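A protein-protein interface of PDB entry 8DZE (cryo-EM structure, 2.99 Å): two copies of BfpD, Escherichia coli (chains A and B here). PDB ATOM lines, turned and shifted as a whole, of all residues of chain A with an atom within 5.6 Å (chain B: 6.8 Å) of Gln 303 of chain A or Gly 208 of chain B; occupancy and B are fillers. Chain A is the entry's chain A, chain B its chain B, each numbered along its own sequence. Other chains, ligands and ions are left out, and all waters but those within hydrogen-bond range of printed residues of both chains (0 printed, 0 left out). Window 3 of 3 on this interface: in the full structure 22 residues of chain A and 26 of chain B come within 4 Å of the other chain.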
ATOM      1  N   SER A 289      10.500 -26.158 -17.062  1.00  0.00           N
ATOM      2  CA  SER A 289      11.687 -26.611 -16.350  1.00  0.00           C
ATOM      3  C   SER A 289      12.285 -25.442 -15.581  1.00  0.00           C
ATOM      4  O   SER A 289      12.608 -24.408 -16.172  1.00  0.00           O
ATOM      5  CB  SER A 289      12.721 -27.204 -17.311  1.00  0.00           C
ATOM      6  OG  SER A 289      12.124 -28.153 -18.176  1.00  0.00           O
ATOM      7  N   GLU A 291      15.407 -24.670 -13.539  1.00  0.00           N
ATOM      8  CA  GLU A 291      16.763 -24.974 -13.091  1.00  0.00           C
ATOM      9  C   GLU A 291      17.531 -23.665 -12.984  1.00  0.00           C
ATOM     10  O   GLU A 291      17.737 -22.981 -13.994  1.00  0.00           O
ATOM     11  CB  GLU A 291      17.456 -25.942 -14.049  1.00  0.00           C
ATOM     12  CG  GLU A 291      17.049 -27.395 -13.871  1.00  0.00           C
ATOM     13  CD  GLU A 291      15.863 -27.776 -14.732  1.00  0.00           C
ATOM     14  OE1 GLU A 291      15.738 -27.230 -15.848  1.00  0.00           O
ATOM     15  OE2 GLU A 291      15.056 -28.622 -14.296  1.00  0.00           O
ATOM     16  N   PRO A 293      20.893 -23.222 -12.180  1.00  0.00           N
ATOM     17  CA  PRO A 293      22.056 -23.337 -13.066  1.00  0.00           C
ATOM     18  C   PRO A 293      21.685 -24.041 -14.359  1.00  0.00           C
ATOM     19  O   PRO A 293      21.264 -25.208 -14.340  1.00  0.00           O
ATOM     20  CB  PRO A 293      23.058 -24.165 -12.244  1.00  0.00           C
ATOM     21  CG  PRO A 293      22.310 -24.640 -11.018  1.00  0.00           C
ATOM     22  CD  PRO A 293      20.864 -24.361 -11.242  1.00  0.00           C
ATOM     23  N   PRO A 294      21.824 -23.370 -15.506  1.00  0.00           N
ATOM     24  CA  PRO A 294      21.530 -24.036 -16.783  1.00  0.00           C
ATOM     25  C   PRO A 294      22.575 -25.083 -17.135  1.00  0.00           C
ATOM     26  O   PRO A 294      23.697 -24.744 -17.522  1.00  0.00           O
ATOM     27  CB  PRO A 294      21.533 -22.881 -17.794  1.00  0.00           C
ATOM     28  CG  PRO A 294      21.350 -21.642 -16.973  1.00  0.00           C
ATOM     29  CD  PRO A 294      22.043 -21.926 -15.678  1.00  0.00           C
ATOM     30  N   GLU A 295      22.217 -26.359 -17.007  1.00  0.00           N
ATOM     31  CA  GLU A 295      23.119 -27.464 -17.310  1.00  0.00           C
ATOM     32  C   GLU A 295      22.427 -28.411 -18.276  1.00  0.00           C
ATOM     33  O   GLU A 295      21.332 -28.902 -17.982  1.00  0.00           O
ATOM     34  CB  GLU A 295      23.533 -28.206 -16.034  1.00  0.00           C
ATOM     35  CG  GLU A 295      24.285 -29.502 -16.285  1.00  0.00           C
ATOM     36  CD  GLU A 295      23.493 -30.726 -15.867  1.00  0.00           C
ATOM     37  OE1 GLU A 295      22.861 -30.688 -14.791  1.00  0.00           O
ATOM     38  OE2 GLU A 295      23.505 -31.728 -16.614  1.00  0.00           O
ATOM     39  N   TYR A 296      23.064 -28.641 -19.433  1.00  0.00           N
ATOM     40  CA  TYR A 296      22.627 -29.562 -20.484  1.00  0.00           C
ATOM     41  C   TYR A 296      21.340 -29.110 -21.171  1.00  0.00           C
ATOM     42  O   TYR A 296      20.515 -28.408 -20.578  1.00  0.00           O
ATOM     43  CB  TYR A 296      22.462 -30.986 -19.937  1.00  0.00           C
ATOM     44  N   ILE A 298      17.631 -29.241 -22.468  1.00  0.00           N
ATOM     45  CA  ILE A 298      16.451 -29.806 -21.827  1.00  0.00           C
ATOM     46  C   ILE A 298      15.191 -29.407 -22.585  1.00  0.00           C
ATOM     47  O   ILE A 298      14.807 -30.060 -23.556  1.00  0.00           O
ATOM     48  CB  ILE A 298      16.367 -29.372 -20.351  1.00  0.00           C
ATOM     49  CG1 ILE A 298      15.516 -30.358 -19.548  1.00  0.00           C
ATOM     50  CG2 ILE A 298      15.807 -27.960 -20.239  1.00  0.00           C
ATOM     51  CD1 ILE A 298      15.742 -30.283 -18.055  1.00  0.00           C
ATOM     52  N   THR A 301      10.327 -27.167 -23.728  1.00  0.00           N
ATOM     53  CA  THR A 301      10.046 -26.616 -22.407  1.00  0.00           C
ATOM     54  C   THR A 301      10.533 -25.180 -22.279  1.00  0.00           C
ATOM     55  O   THR A 301      11.252 -24.674 -23.141  1.00  0.00           O
ATOM     56  CB  THR A 301      10.700 -27.453 -21.292  1.00  0.00           C
ATOM     57  OG1 THR A 301      10.266 -26.974 -20.013  1.00  0.00           O
ATOM     58  CG2 THR A 301      12.215 -27.359 -21.376  1.00  0.00           C
ATOM     59  N   ALA A 302      10.132 -24.530 -21.192  1.00  0.00           N
ATOM     60  CA  ALA A 302      10.609 -23.198 -20.848  1.00  0.00           C
ATOM     61  C   ALA A 302      11.660 -23.346 -19.755  1.00  0.00           C
ATOM     62  O   ALA A 302      11.339 -23.728 -18.626  1.00  0.00           O
ATOM     63  CB  ALA A 302       9.458 -22.303 -20.393  1.00  0.00           C
ATOM     64  N   GLN A 303      12.913 -23.048 -20.091  1.00  0.00           N
ATOM     65  CA  GLN A 303      14.024 -23.182 -19.152  1.00  0.00           C
ATOM     66  C   GLN A 303      14.084 -21.918 -18.306  1.00  0.00           C
ATOM     67  O   GLN A 303      14.631 -20.896 -18.728  1.00  0.00           O
ATOM     68  CB  GLN A 303      15.333 -23.425 -19.895  1.00  0.00           C
ATOM     69  CG  GLN A 303      16.498 -23.796 -18.993  1.00  0.00           C
ATOM     70  CD  GLN A 303      17.748 -24.156 -19.773  1.00  0.00           C
ATOM     71  OE1 GLN A 303      17.774 -24.069 -21.001  1.00  0.00           O
ATOM     72  NE2 GLN A 303      18.792 -24.562 -19.061  1.00  0.00           N
ATOM     73  N   LEU A 304      13.519 -21.987 -17.103  1.00  0.00           N
ATOM     74  CA  LEU A 304      13.472 -20.836 -16.212  1.00  0.00           C
ATOM     75  C   LEU A 304      14.760 -20.761 -15.404  1.00  0.00           C
ATOM     76  O   LEU A 304      15.077 -21.713 -14.679  1.00  0.00           O
ATOM     77  CB  LEU A 304      12.276 -20.928 -15.277  1.00  0.00           C
ATOM     78  CG  LEU A 304      10.958 -20.287 -15.726  1.00  0.00           C
ATOM     79  CD1 LEU A 304      10.342 -21.027 -16.906  1.00  0.00           C
ATOM     80  CD2 LEU A 304       9.978 -20.230 -14.565  1.00  0.00           C
ATOM     81  N   PRO A 305      15.529 -19.666 -15.494  1.00  0.00           N
ATOM     82  CA  PRO A 305      16.775 -19.517 -14.736  1.00  0.00           C
ATOM     83  C   PRO A 305      16.530 -19.212 -13.261  1.00  0.00           C
ATOM     84  O   PRO A 305      17.373 -18.568 -12.636  1.00  0.00           O
ATOM     85  CB  PRO A 305      17.463 -18.339 -15.428  1.00  0.00           C
ATOM     86  CG  PRO A 305      16.342 -17.528 -15.974  1.00  0.00           C
ATOM     87  CD  PRO A 305      15.265 -18.504 -16.361  1.00  0.00           C
ATOM     88  N   VAL B 130       9.907 -16.726 -26.935  1.00  0.00           N
ATOM     89  CA  VAL B 130      10.875 -16.037 -27.784  1.00  0.00           C
ATOM     90  C   VAL B 130      12.235 -16.698 -27.611  1.00  0.00           C
ATOM     91  O   VAL B 130      12.732 -16.827 -26.485  1.00  0.00           O
ATOM     92  CB  VAL B 130      10.946 -14.536 -27.458  1.00  0.00           C
ATOM     93  CG1 VAL B 130      11.511 -13.769 -28.642  1.00  0.00           C
ATOM     94  CG2 VAL B 130       9.570 -14.006 -27.088  1.00  0.00           C
ATOM     95  N   TYR B 131      12.835 -17.116 -28.728  1.00  0.00           N
ATOM     96  CA  TYR B 131      14.141 -17.768 -28.730  1.00  0.00           C
ATOM     97  C   TYR B 131      15.196 -16.948 -29.470  1.00  0.00           C
ATOM     98  O   TYR B 131      16.243 -17.490 -29.840  1.00  0.00           O
ATOM     99  CB  TYR B 131      14.041 -19.165 -29.347  1.00  0.00           C
ATOM    100  CG  TYR B 131      13.171 -20.129 -28.575  1.00  0.00           C
ATOM    101  CD1 TYR B 131      13.482 -20.483 -27.268  1.00  0.00           C
ATOM    102  CD2 TYR B 131      12.041 -20.690 -29.156  1.00  0.00           C
ATOM    103  CE1 TYR B 131      12.690 -21.368 -26.561  1.00  0.00           C
ATOM    104  CE2 TYR B 131      11.242 -21.576 -28.456  1.00  0.00           C
ATOM    105  CZ  TYR B 131      11.571 -21.911 -27.160  1.00  0.00           C
ATOM    106  OH  TYR B 131      10.780 -22.791 -26.460  1.00  0.00           O
ATOM    107  N   TYR B 179      10.927 -11.586 -13.528  1.00  0.00           N
ATOM    108  CA  TYR B 179       9.563 -12.075 -13.678  1.00  0.00           C
ATOM    109  C   TYR B 179       8.568 -10.943 -13.461  1.00  0.00           C
ATOM    110  O   TYR B 179       8.789 -10.054 -12.633  1.00  0.00           O
ATOM    111  CB  TYR B 179       9.291 -13.205 -12.683  1.00  0.00           C
ATOM    112  CG  TYR B 179      10.100 -14.459 -12.927  1.00  0.00           C
ATOM    113  CD1 TYR B 179      11.387 -14.588 -12.422  1.00  0.00           C
ATOM    114  CD2 TYR B 179       9.571 -15.518 -13.651  1.00  0.00           C
ATOM    115  CE1 TYR B 179      12.129 -15.732 -12.643  1.00  0.00           C
ATOM    116  CE2 TYR B 179      10.304 -16.667 -13.874  1.00  0.00           C
ATOM    117  CZ  TYR B 179      11.583 -16.769 -13.368  1.00  0.00           C
ATOM    118  OH  TYR B 179      12.316 -17.911 -13.589  1.00  0.00           O
ATOM    119  N   PRO B 206      11.365 -14.752 -17.797  1.00  0.00           N
ATOM    120  CA  PRO B 206      12.591 -14.830 -18.597  1.00  0.00           C
ATOM    121  C   PRO B 206      12.779 -16.223 -19.174  1.00  0.00           C
ATOM    122  O   PRO B 206      12.294 -17.219 -18.631  1.00  0.00           O
ATOM    123  CB  PRO B 206      13.695 -14.489 -17.590  1.00  0.00           C
ATOM    124  CG  PRO B 206      13.108 -14.844 -16.265  1.00  0.00           C
ATOM    125  CD  PRO B 206      11.654 -14.495 -16.377  1.00  0.00           C
ATOM    126  N   LEU B 207      13.499 -16.286 -20.292  1.00  0.00           N
ATOM    127  CA  LEU B 207      13.699 -17.550 -20.996  1.00  0.00           C
ATOM    128  C   LEU B 207      15.105 -17.562 -21.581  1.00  0.00           C
ATOM    129  O   LEU B 207      15.350 -16.928 -22.611  1.00  0.00           O
ATOM    130  CB  LEU B 207      12.649 -17.736 -22.087  1.00  0.00           C
ATOM    131  CG  LEU B 207      12.728 -19.019 -22.912  1.00  0.00           C
ATOM    132  CD1 LEU B 207      12.545 -20.231 -22.021  1.00  0.00           C
ATOM    133  CD2 LEU B 207      11.684 -19.001 -24.015  1.00  0.00           C
ATOM    134  N   GLY B 208      16.009 -18.296 -20.940  1.00  0.00           N
ATOM    135  CA  GLY B 208      17.378 -18.368 -21.430  1.00  0.00           C
ATOM    136  C   GLY B 208      18.073 -17.026 -21.335  1.00  0.00           C
ATOM    137  O   GLY B 208      18.066 -16.366 -20.289  1.00  0.00           O
ATOM    138  N   GLN B 209      18.685 -16.609 -22.440  1.00  0.00           N
ATOM    139  CA  GLN B 209      19.394 -15.336 -22.528  1.00  0.00           C
ATOM    140  C   GLN B 209      18.626 -14.421 -23.475  1.00  0.00           C
ATOM    141  O   GLN B 209      18.598 -14.656 -24.688  1.00  0.00           O
ATOM    142  CB  GLN B 209      20.829 -15.544 -23.005  1.00  0.00           C
ATOM    143  N   GLY B 210      18.012 -13.382 -22.920  1.00  0.00           N
ATOM    144  CA  GLY B 210      17.260 -12.426 -23.715  1.00  0.00           C
ATOM    145  C   GLY B 210      16.010 -12.981 -24.363  1.00  0.00           C
ATOM    146  O   GLY B 210      15.668 -12.580 -25.483  1.00  0.00           O
ATOM    147  N   GLY B 211      15.312 -13.888 -23.687  1.00  0.00           N
ATOM    148  CA  GLY B 211      14.078 -14.440 -24.210  1.00  0.00           C
ATOM    149  C   GLY B 211      12.908 -14.200 -23.280  1.00  0.00           C
ATOM    150  O   GLY B 211      13.102 -13.944 -22.088  1.00  0.00           O
ATOM    151  N   ARG B 212      11.689 -14.277 -23.807  1.00  0.00           N
ATOM    152  CA  ARG B 212      10.496 -13.974 -23.033  1.00  0.00           C
ATOM    153  C   ARG B 212       9.464 -15.081 -23.198  1.00  0.00           C
ATOM    154  O   ARG B 212       9.353 -15.705 -24.257  1.00  0.00           O
ATOM    155  CB  ARG B 212       9.895 -12.623 -23.448  1.00  0.00           C
ATOM    156  CG  ARG B 212       9.247 -11.847 -22.310  1.00  0.00           C
ATOM    157  CD  ARG B 212      10.155 -11.781 -21.096  1.00  0.00           C
ATOM    158  NE  ARG B 212       9.468 -11.252 -19.923  1.00  0.00           N
ATOM    159  CZ  ARG B 212      10.077 -10.912 -18.795  1.00  0.00           C
ATOM    160  NH1 ARG B 212      11.374 -11.095 -18.630  1.00  0.00           N
ATOM    161  NH2 ARG B 212       9.364 -10.384 -17.804  1.00  0.00           N
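Of the 12 printed residues of chain A, 5 touch a printed residue of chain B.
Of the 10 printed residues of chain B, 5 touch a printed residue of chain A.
Printed residues of chain B that touch a printed residue of chain A: Tyr 131, Tyr 179, Pro 206, Leu 207 and Gly 208.
Among the printed residues, no Asp or Glu carboxylate lies within 4 Å of a Lys or Arg side-chain nitrogen of the other chain.
OG of Ser 289 of chain A sits at hydrogen-bond distance from OG1 of Thr 301 of chain A, 2.9 Å away.
The backbone NH of Ser 289 of chain A sits at hydrogen-bond distance from the backbone carbonyl oxygen of Ala 302 of chain A (3.0 Å).
The backbone NH of Leu 304 of chain A is in hydrogen-bond range of the backbone carbonyl oxygen of Ser 289 of chain A (2.7 Å).
N of Glu 291 of chain A lies within hydrogen-bond range of O of Leu 304 of chain A, at 3.2 Å.
No position is printed for both chains.
Of the 6 pairs that touch across the chains among the printed residues, none has its exchanged pair printed and touching as well.
Among the printed residues, merely in contact across the chains: Thr 301 of chain A with Tyr 131 of chain B, Ala 302 of chain A with Leu 207 of chain B, Gln 303 of chain A with Leu 207 of chain B, Gln 303 of chain A with Gly 208 of chain B, Leu 304 of chain A with Tyr 179 of chain B and Pro 305 of chain A with Pro 206 of chain B.
Printed residues of chain B within 4 Å of Thr 301 of chain A: Tyr 131.
Printed residues of chain B within 4 Å of Leu 304 of chain A: Tyr 179 (3.4 Å).
Of the printed residues of chain A, Tyr 131 of chain B touches Thr 301 (3.8 Å).
Printed residues of chain A within 4 Å of Leu 207 of chain B: Ala 302 and Gln 303.
Of chain A, only Gln 303 (3.7 Å) comes within 4 Å of Gly 208 of chain B.
The nearest residue of chain B that does not touch Gln 303 of chain A is Pro 206 of chain B (4.4 Å).
The nearest residue of chain A that does not touch Gly 208 of chain B is Pro 305 of chain A (4.6 Å).
The nearest printed residue of chain B that does not touch Pro 305 of chain A is Tyr 179 of chain B (4.1 Å).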
